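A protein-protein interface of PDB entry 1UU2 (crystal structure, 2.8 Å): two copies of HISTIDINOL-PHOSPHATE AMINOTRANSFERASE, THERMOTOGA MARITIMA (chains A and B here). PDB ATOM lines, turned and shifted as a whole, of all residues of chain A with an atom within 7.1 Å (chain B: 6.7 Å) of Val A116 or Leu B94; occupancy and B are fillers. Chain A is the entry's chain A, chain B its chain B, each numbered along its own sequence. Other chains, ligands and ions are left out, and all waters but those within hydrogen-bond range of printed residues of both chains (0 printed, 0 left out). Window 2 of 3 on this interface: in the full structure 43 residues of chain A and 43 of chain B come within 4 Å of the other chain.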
ATOM      1  N   ILE A  89      25.517   4.131  23.438  1.00  0.00           N
ATOM      2  CA  ILE A  89      25.106   5.085  22.420  1.00  0.00           C
ATOM      3  C   ILE A  89      23.595   4.940  22.243  1.00  0.00           C
ATOM      4  O   ILE A  89      22.845   5.917  22.272  1.00  0.00           O
ATOM      5  CB  ILE A  89      25.781   4.764  21.069  1.00  0.00           C
ATOM      6  CG1 ILE A  89      27.308   4.777  21.224  1.00  0.00           C
ATOM      7  CG2 ILE A  89      25.312   5.745  20.003  1.00  0.00           C
ATOM      8  CD1 ILE A  89      27.882   6.112  21.645  1.00  0.00           C
ATOM      9  N   TYR A  90      23.176   3.693  22.064  1.00  0.00           N
ATOM     10  CA  TYR A  90      21.783   3.322  21.871  1.00  0.00           C
ATOM     11  C   TYR A  90      20.858   3.972  22.897  1.00  0.00           C
ATOM     12  O   TYR A  90      20.000   4.780  22.541  1.00  0.00           O
ATOM     13  CB  TYR A  90      21.669   1.798  21.941  1.00  0.00           C
ATOM     14  CG  TYR A  90      20.403   1.221  21.357  1.00  0.00           C
ATOM     15  CD1 TYR A  90      19.204   1.252  22.066  1.00  0.00           C
ATOM     16  CD2 TYR A  90      20.410   0.622  20.097  1.00  0.00           C
ATOM     17  CE1 TYR A  90      18.044   0.697  21.536  1.00  0.00           C
ATOM     18  CE2 TYR A  90      19.261   0.067  19.560  1.00  0.00           C
ATOM     19  CZ  TYR A  90      18.082   0.107  20.284  1.00  0.00           C
ATOM     20  OH  TYR A  90      16.940  -0.450  19.757  1.00  0.00           O
ATOM     21  N   VAL A  91      21.031   3.622  24.169  1.00  0.00           N
ATOM     22  CA  VAL A  91      20.188   4.184  25.221  1.00  0.00           C
ATOM     23  C   VAL A  91      20.304   5.698  25.292  1.00  0.00           C
ATOM     24  O   VAL A  91      19.335   6.387  25.587  1.00  0.00           O
ATOM     25  CB  VAL A  91      20.542   3.608  26.613  1.00  0.00           C
ATOM     26  CG1 VAL A  91      20.181   2.134  26.684  1.00  0.00           C
ATOM     27  CG2 VAL A  91      22.015   3.802  26.883  1.00  0.00           C
ATOM     28  N   MET A  92      21.491   6.218  25.013  1.00  0.00           N
ATOM     29  CA  MET A  92      21.708   7.657  25.067  1.00  0.00           C
ATOM     30  C   MET A  92      20.805   8.429  24.106  1.00  0.00           C
ATOM     31  O   MET A  92      20.320   9.515  24.431  1.00  0.00           O
ATOM     32  CB  MET A  92      23.175   7.976  24.782  1.00  0.00           C
ATOM     33  CG  MET A  92      23.755   8.975  25.749  1.00  0.00           C
ATOM     34  SD  MET A  92      25.239   8.365  26.528  1.00  0.00           S
ATOM     35  CE  MET A  92      26.237   9.874  26.515  1.00  0.00           C
ATOM     36  N   MET A  93      20.576   7.869  22.924  1.00  0.00           N
ATOM     37  CA  MET A  93      19.715   8.520  21.950  1.00  0.00           C
ATOM     38  C   MET A  93      18.262   8.442  22.411  1.00  0.00           C
ATOM     39  O   MET A  93      17.380   9.072  21.829  1.00  0.00           O
ATOM     40  CB  MET A  93      19.872   7.855  20.587  1.00  0.00           C
ATOM     41  CG  MET A  93      21.318   7.753  20.150  1.00  0.00           C
ATOM     42  SD  MET A  93      21.524   7.328  18.420  1.00  0.00           S
ATOM     43  CE  MET A  93      23.081   8.160  18.055  1.00  0.00           C
ATOM     44  N   LEU A  94      18.020   7.663  23.462  1.00  0.00           N
ATOM     45  CA  LEU A  94      16.678   7.504  24.016  1.00  0.00           C
ATOM     46  C   LEU A  94      16.421   8.516  25.120  1.00  0.00           C
ATOM     47  O   LEU A  94      15.275   8.817  25.437  1.00  0.00           O
ATOM     48  CB  LEU A  94      16.500   6.107  24.602  1.00  0.00           C
ATOM     49  CG  LEU A  94      16.293   4.923  23.664  1.00  0.00           C
ATOM     50  CD1 LEU A  94      16.444   3.638  24.455  1.00  0.00           C
ATOM     51  CD2 LEU A  94      14.918   4.995  23.023  1.00  0.00           C
ATOM     52  N   MET A  95      17.495   9.042  25.695  1.00  0.00           N
ATOM     53  CA  MET A  95      17.387   9.988  26.796  1.00  0.00           C
ATOM     54  C   MET A  95      17.218  11.453  26.411  1.00  0.00           C
ATOM     55  O   MET A  95      16.548  12.206  27.116  1.00  0.00           O
ATOM     56  CB  MET A  95      18.607   9.844  27.708  1.00  0.00           C
ATOM     57  CG  MET A  95      18.903   8.413  28.119  1.00  0.00           C
ATOM     58  SD  MET A  95      19.998   8.323  29.544  1.00  0.00           S
ATOM     59  CE  MET A  95      21.554   8.624  28.787  1.00  0.00           C
ATOM     60  N   ILE A 111      22.485   4.822  12.164  1.00  0.00           N
ATOM     61  CA  ILE A 111      21.701   3.602  12.162  1.00  0.00           C
ATOM     62  C   ILE A 111      20.878   3.464  13.432  1.00  0.00           C
ATOM     63  O   ILE A 111      19.689   3.144  13.373  1.00  0.00           O
ATOM     64  CB  ILE A 111      22.604   2.362  12.024  1.00  0.00           C
ATOM     65  CG1 ILE A 111      23.367   2.422  10.700  1.00  0.00           C
ATOM     66  CG2 ILE A 111      21.772   1.100  12.102  1.00  0.00           C
ATOM     67  CD1 ILE A 111      22.482   2.631   9.483  1.00  0.00           C
ATOM     68  N   PHE A 112      21.508   3.702  14.578  1.00  0.00           N
ATOM     69  CA  PHE A 112      20.809   3.578  15.851  1.00  0.00           C
ATOM     70  C   PHE A 112      19.814   4.702  16.071  1.00  0.00           C
ATOM     71  O   PHE A 112      18.751   4.488  16.646  1.00  0.00           O
ATOM     72  CB  PHE A 112      21.800   3.534  17.021  1.00  0.00           C
ATOM     73  CG  PHE A 112      22.675   2.312  17.032  1.00  0.00           C
ATOM     74  CD1 PHE A 112      22.268   1.140  16.407  1.00  0.00           C
ATOM     75  CD2 PHE A 112      23.901   2.329  17.680  1.00  0.00           C
ATOM     76  CE1 PHE A 112      23.070   0.004  16.425  1.00  0.00           C
ATOM     77  CE2 PHE A 112      24.712   1.197  17.704  1.00  0.00           C
ATOM     78  CZ  PHE A 112      24.293   0.033  17.074  1.00  0.00           C
ATOM     79  N   ALA A 113      20.164   5.899  15.617  1.00  0.00           N
ATOM     80  CA  ALA A 113      19.281   7.047  15.769  1.00  0.00           C
ATOM     81  C   ALA A 113      17.952   6.734  15.088  1.00  0.00           C
ATOM     82  O   ALA A 113      16.885   6.977  15.647  1.00  0.00           O
ATOM     83  CB  ALA A 113      19.916   8.283  15.147  1.00  0.00           C
ATOM     84  N   LYS A 114      18.025   6.193  13.876  1.00  0.00           N
ATOM     85  CA  LYS A 114      16.828   5.837  13.128  1.00  0.00           C
ATOM     86  C   LYS A 114      16.089   4.711  13.839  1.00  0.00           C
ATOM     87  O   LYS A 114      14.903   4.831  14.146  1.00  0.00           O
ATOM     88  CB  LYS A 114      17.200   5.380  11.717  1.00  0.00           C
ATOM     89  CG  LYS A 114      17.569   6.493  10.759  1.00  0.00           C
ATOM     90  CD  LYS A 114      17.987   5.916   9.414  1.00  0.00           C
ATOM     91  CE  LYS A 114      17.803   6.929   8.294  1.00  0.00           C
ATOM     92  NZ  LYS A 114      18.502   8.214   8.571  1.00  0.00           N
ATOM     93  N   ALA A 115      16.808   3.619  14.092  1.00  0.00           N
ATOM     94  CA  ALA A 115      16.258   2.446  14.760  1.00  0.00           C
ATOM     95  C   ALA A 115      15.464   2.834  16.001  1.00  0.00           C
ATOM     96  O   ALA A 115      14.272   2.549  16.108  1.00  0.00           O
ATOM     97  CB  ALA A 115      17.387   1.493  15.139  1.00  0.00           C
ATOM     98  N   VAL A 116      16.137   3.478  16.942  1.00  0.00           N
ATOM     99  CA  VAL A 116      15.501   3.920  18.173  1.00  0.00           C
ATOM    100  C   VAL A 116      14.345   4.873  17.870  1.00  0.00           C
ATOM    101  O   VAL A 116      13.342   4.890  18.584  1.00  0.00           O
ATOM    102  CB  VAL A 116      16.538   4.610  19.097  1.00  0.00           C
ATOM    103  CG1 VAL A 116      15.860   5.602  20.021  1.00  0.00           C
ATOM    104  CG2 VAL A 116      17.275   3.555  19.911  1.00  0.00           C
ATOM    105  N   GLY A 117      14.490   5.656  16.804  1.00  0.00           N
ATOM    106  CA  GLY A 117      13.452   6.601  16.429  1.00  0.00           C
ATOM    107  C   GLY A 117      13.693   8.012  16.946  1.00  0.00           C
ATOM    108  O   GLY A 117      12.778   8.834  16.982  1.00  0.00           O
ATOM    109  N   ALA A 118      14.929   8.291  17.344  1.00  0.00           N
ATOM    110  CA  ALA A 118      15.296   9.604  17.855  1.00  0.00           C
ATOM    111  C   ALA A 118      15.529  10.638  16.745  1.00  0.00           C
ATOM    112  O   ALA A 118      15.863  10.298  15.607  1.00  0.00           O
ATOM    113  CB  ALA A 118      16.543   9.489  18.722  1.00  0.00           C
ATOM    114  N   LYS A 119      15.352  11.905  17.096  1.00  0.00           N
ATOM    115  CA  LYS A 119      15.548  13.004  16.162  1.00  0.00           C
ATOM    116  C   LYS A 119      17.040  13.306  16.060  1.00  0.00           C
ATOM    117  O   LYS A 119      17.704  13.536  17.073  1.00  0.00           O
ATOM    118  CB  LYS A 119      14.809  14.245  16.666  1.00  0.00           C
ATOM    119  CG  LYS A 119      14.868  15.438  15.724  1.00  0.00           C
ATOM    120  CD  LYS A 119      14.280  16.690  16.365  1.00  0.00           C
ATOM    121  CE  LYS A 119      12.845  16.470  16.834  1.00  0.00           C
ATOM    122  NZ  LYS A 119      12.276  17.658  17.537  1.00  0.00           N
ATOM    123  N   ILE B  89      11.518  -7.668  24.794  1.00  0.00           N
ATOM    124  CA  ILE B  89      10.463  -6.792  25.288  1.00  0.00           C
ATOM    125  C   ILE B  89      10.851  -5.347  24.973  1.00  0.00           C
ATOM    126  O   ILE B  89      10.199  -4.665  24.186  1.00  0.00           O
ATOM    127  CB  ILE B  89      10.291  -6.928  26.833  1.00  0.00           C
ATOM    128  CG1 ILE B  89       9.514  -8.202  27.177  1.00  0.00           C
ATOM    129  CG2 ILE B  89       9.565  -5.708  27.391  1.00  0.00           C
ATOM    130  CD1 ILE B  89      10.196  -9.471  26.758  1.00  0.00           C
ATOM    131  N   TYR B  90      11.931  -4.905  25.603  1.00  0.00           N
ATOM    132  CA  TYR B  90      12.471  -3.561  25.451  1.00  0.00           C
ATOM    133  C   TYR B  90      12.407  -3.033  24.007  1.00  0.00           C
ATOM    134  O   TYR B  90      11.896  -1.943  23.761  1.00  0.00           O
ATOM    135  CB  TYR B  90      13.910  -3.579  25.967  1.00  0.00           C
ATOM    136  CG  TYR B  90      14.509  -2.232  26.294  1.00  0.00           C
ATOM    137  CD1 TYR B  90      15.007  -1.402  25.292  1.00  0.00           C
ATOM    138  CD2 TYR B  90      14.639  -1.817  27.619  1.00  0.00           C
ATOM    139  CE1 TYR B  90      15.635  -0.196  25.602  1.00  0.00           C
ATOM    140  CE2 TYR B  90      15.263  -0.612  27.939  1.00  0.00           C
ATOM    141  CZ  TYR B  90      15.765   0.189  26.925  1.00  0.00           C
ATOM    142  OH  TYR B  90      16.434   1.349  27.237  1.00  0.00           O
ATOM    143  N   VAL B  91      12.915  -3.812  23.054  1.00  0.00           N
ATOM    144  CA  VAL B  91      12.909  -3.397  21.655  1.00  0.00           C
ATOM    145  C   VAL B  91      11.523  -3.383  21.020  1.00  0.00           C
ATOM    146  O   VAL B  91      11.186  -2.445  20.294  1.00  0.00           O
ATOM    147  CB  VAL B  91      13.803  -4.301  20.787  1.00  0.00           C
ATOM    148  CG1 VAL B  91      15.272  -4.093  21.131  1.00  0.00           C
ATOM    149  CG2 VAL B  91      13.408  -5.738  20.990  1.00  0.00           C
ATOM    150  N   MET B  92      10.721  -4.416  21.272  1.00  0.00           N
ATOM    151  CA  MET B  92       9.389  -4.460  20.682  1.00  0.00           C
ATOM    152  C   MET B  92       8.639  -3.178  20.979  1.00  0.00           C
ATOM    153  O   MET B  92       8.097  -2.553  20.072  1.00  0.00           O
ATOM    154  CB  MET B  92       8.591  -5.656  21.196  1.00  0.00           C
ATOM    155  CG  MET B  92       9.082  -6.986  20.653  1.00  0.00           C
ATOM    156  SD  MET B  92       8.066  -8.378  21.164  1.00  0.00           S
ATOM    157  CE  MET B  92       6.983  -8.534  19.750  1.00  0.00           C
ATOM    158  N   MET B  93       8.626  -2.776  22.243  1.00  0.00           N
ATOM    159  CA  MET B  93       7.937  -1.552  22.639  1.00  0.00           C
ATOM    160  C   MET B  93       8.397  -0.332  21.843  1.00  0.00           C
ATOM    161  O   MET B  93       7.687   0.666  21.766  1.00  0.00           O
ATOM    162  CB  MET B  93       8.151  -1.282  24.125  1.00  0.00           C
ATOM    163  CG  MET B  93       7.660  -2.388  25.043  1.00  0.00           C
ATOM    164  SD  MET B  93       7.756  -1.876  26.763  1.00  0.00           S
ATOM    165  CE  MET B  93       9.382  -1.136  26.745  1.00  0.00           C
ATOM    166  N   LEU B  94       9.591  -0.414  21.266  1.00  0.00           N
ATOM    167  CA  LEU B  94      10.140   0.678  20.473  1.00  0.00           C
ATOM    168  C   LEU B  94       9.552   0.654  19.076  1.00  0.00           C
ATOM    169  O   LEU B  94       9.473   1.686  18.419  1.00  0.00           O
ATOM    170  CB  LEU B  94      11.659   0.545  20.345  1.00  0.00           C
ATOM    171  CG  LEU B  94      12.621   0.919  21.474  1.00  0.00           C
ATOM    172  CD1 LEU B  94      13.932   0.193  21.257  1.00  0.00           C
ATOM    173  CD2 LEU B  94      12.854   2.414  21.501  1.00  0.00           C
ATOM    174  N   MET B  95       9.140  -0.531  18.629  1.00  0.00           N
ATOM    175  CA  MET B  95       8.600  -0.699  17.280  1.00  0.00           C
ATOM    176  C   MET B  95       7.088  -0.866  17.142  1.00  0.00           C
ATOM    177  O   MET B  95       6.613  -1.520  16.212  1.00  0.00           O
ATOM    178  CB  MET B  95       9.315  -1.870  16.585  1.00  0.00           C
ATOM    179  CG  MET B  95       9.208  -3.213  17.300  1.00  0.00           C
ATOM    180  SD  MET B  95      10.411  -4.427  16.676  1.00  0.00           S
ATOM    181  CE  MET B  95       9.691  -4.849  15.116  1.00  0.00           C
ATOM    182  N   PHE B  96       6.339  -0.270  18.063  1.00  0.00           N
ATOM    183  CA  PHE B  96       4.879  -0.330  18.029  1.00  0.00           C
ATOM    184  C   PHE B  96       4.339   0.961  18.620  1.00  0.00           C
ATOM    185  O   PHE B  96       4.879   1.474  19.600  1.00  0.00           O
ATOM    186  CB  PHE B  96       4.359  -1.538  18.819  1.00  0.00           C
ATOM    187  CG  PHE B  96       4.523  -2.849  18.099  1.00  0.00           C
ATOM    188  CD1 PHE B  96       3.769  -3.131  16.960  1.00  0.00           C
ATOM    189  CD2 PHE B  96       5.444  -3.793  18.543  1.00  0.00           C
ATOM    190  CE1 PHE B  96       3.929  -4.332  16.273  1.00  0.00           C
ATOM    191  CE2 PHE B  96       5.612  -4.997  17.863  1.00  0.00           C
ATOM    192  CZ  PHE B  96       4.851  -5.266  16.724  1.00  0.00           C
ATOM    193  N   ASP B  97       3.276   1.487  18.023  1.00  0.00           N
ATOM    194  CA  ASP B  97       2.698   2.738  18.490  1.00  0.00           C
ATOM    195  C   ASP B  97       2.346   2.692  19.977  1.00  0.00           C
ATOM    196  O   ASP B  97       2.613   3.643  20.718  1.00  0.00           O
ATOM    197  CB  ASP B  97       1.462   3.088  17.649  1.00  0.00           C
ATOM    198  CG  ASP B  97       1.055   4.550  17.787  1.00  0.00           C
ATOM    199  OD1 ASP B  97       0.379   4.904  18.777  1.00  0.00           O
ATOM    200  OD2 ASP B  97       1.426   5.352  16.902  1.00  0.00           O
ATOM    201  N   SER B  99       2.014  -0.016  23.613  1.00  0.00           N
ATOM    202  CA  SER B  99       2.170  -1.287  24.311  1.00  0.00           C
ATOM    203  C   SER B  99       1.103  -1.395  25.382  1.00  0.00           C
ATOM    204  O   SER B  99       0.932  -0.490  26.200  1.00  0.00           O
ATOM    205  CB  SER B  99       3.553  -1.396  24.962  1.00  0.00           C
ATOM    206  OG  SER B  99       4.534  -1.756  24.009  1.00  0.00           O
ATOM    207  N   VAL B 116      11.631   3.712  27.605  1.00  0.00           N
ATOM    208  CA  VAL B 116      11.675   3.834  26.156  1.00  0.00           C
ATOM    209  C   VAL B 116      10.899   5.053  25.668  1.00  0.00           C
ATOM    210  O   VAL B 116      11.091   5.516  24.538  1.00  0.00           O
ATOM    211  CB  VAL B 116      11.112   2.560  25.497  1.00  0.00           C
ATOM    212  CG1 VAL B 116      10.950   2.759  24.007  1.00  0.00           C
ATOM    213  CG2 VAL B 116      12.045   1.391  25.767  1.00  0.00           C
ATOM    214  N   GLY B 117      10.036   5.583  26.531  1.00  0.00           N
ATOM    215  CA  GLY B 117       9.234   6.734  26.156  1.00  0.00           C
ATOM    216  C   GLY B 117       8.093   6.256  25.279  1.00  0.00           C
ATOM    217  O   GLY B 117       7.556   7.001  24.460  1.00  0.00           O
ATOM    218  N   ALA B 118       7.732   4.993  25.462  1.00  0.00           N
ATOM    219  CA  ALA B 118       6.665   4.375  24.698  1.00  0.00           C
ATOM    220  C   ALA B 118       5.302   4.662  25.305  1.00  0.00           C
ATOM    221  O   ALA B 118       5.195   5.047  26.467  1.00  0.00           O
ATOM    222  CB  ALA B 118       6.892   2.867  24.622  1.00  0.00           C
ATOM    223  N   ARG B 226      16.450  -5.289  12.735  1.00  0.00           N
ATOM    224  CA  ARG B 226      16.860  -3.941  12.359  1.00  0.00           C
ATOM    225  C   ARG B 226      16.813  -2.952  13.518  1.00  0.00           C
ATOM    226  O   ARG B 226      17.462  -1.900  13.472  1.00  0.00           O
ATOM    227  CB  ARG B 226      15.986  -3.420  11.213  1.00  0.00           C
ATOM    228  CG  ARG B 226      16.196  -4.154   9.901  1.00  0.00           C
ATOM    229  CD  ARG B 226      15.498  -3.466   8.732  1.00  0.00           C
ATOM    230  NE  ARG B 226      15.811  -4.128   7.465  1.00  0.00           N
ATOM    231  CZ  ARG B 226      17.039  -4.245   6.964  1.00  0.00           C
ATOM    232  NH1 ARG B 226      18.080  -3.743   7.617  1.00  0.00           N
ATOM    233  NH2 ARG B 226      17.229  -4.876   5.815  1.00  0.00           N
ATOM    234  N   VAL B 227      16.059  -3.290  14.560  1.00  0.00           N
ATOM    235  CA  VAL B 227      15.928  -2.409  15.711  1.00  0.00           C
ATOM    236  C   VAL B 227      16.849  -2.795  16.868  1.00  0.00           C
ATOM    237  O   VAL B 227      17.389  -1.927  17.549  1.00  0.00           O
ATOM    238  CB  VAL B 227      14.473  -2.393  16.223  1.00  0.00           C
ATOM    239  CG1 VAL B 227      14.226  -1.136  17.049  1.00  0.00           C
ATOM    240  CG2 VAL B 227      13.506  -2.468  15.054  1.00  0.00           C
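Printed residues of chain A that touch a printed residue of chain B: Tyr A90, Val A91, Leu A94, Ala A115 and Val A116. Hydrophobic or aromatic side chains of chain A that line the printed part of chain B: Tyr A90, Val A91, Leu A94 and Ala A115. Of the 15 printed residues of chain B, 4 touch a printed residue of chain A. Among the printed residues, no Asp or Glu carboxylate lies within 4 Å of a Lys or Arg side-chain nitrogen of the other chain.
Val A116 touches just one residue of chain B: Leu B94. Of chain A, only Tyr A90, Leu A94 and Val A116 come within 4 Å of Leu B94. Printed residues of chain B within 4 Å of Tyr A90: Leu B94 (3.4 Å) and Val B227 (2.7 Å). Printed residues of chain B within 4 Å of Ala A115: Arg B226 (3.8 Å) and Val B227 (3.8 Å). Of the printed residues of chain A, Tyr B90 touches Val A91 (3.9 Å) and Leu A94 (3.6 Å). Of the printed residues of chain A, Val B227 touches Tyr A90 (2.7 Å) and Ala A115 (3.8 Å). Lys A119 touches none of the printed residues of chain B.
O of Val B227 is in hydrogen-bond range of OH of Tyr A90 (2.7 Å).
Tyr A90 touches Leu B94, and with the chains exchanged Leu A94 touches Tyr B90. Val A91 touches Tyr B90, but with the chains exchanged Tyr A90 does not touch Val B91 (4.2 Å). Leu B94 touches its own counterpart, Leu A94. Val A116 touches Leu B94, but with the chains exchanged Leu A94 does not touch Val B116 (4.1 Å). Positions printed for both chains: 89, 90, 91, 92, 93, 94, 95, 116, 117 and 118.
Tyr A90 touches Leu B94 (OH to CD1, 3.4 Å). CG1 of Val A91 touches OH of Tyr B90, at 3.9 Å. Leu A94 touches Tyr B90. CD2 of Leu B94 touches CD2 of Leu A94, at 3.6 Å. Ala A115 touches Arg B226 (CB to O, 3.8 Å). Ala A115 touches Val B227. Val A116 touches Leu B94 (O to CD2, 3.9 Å).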
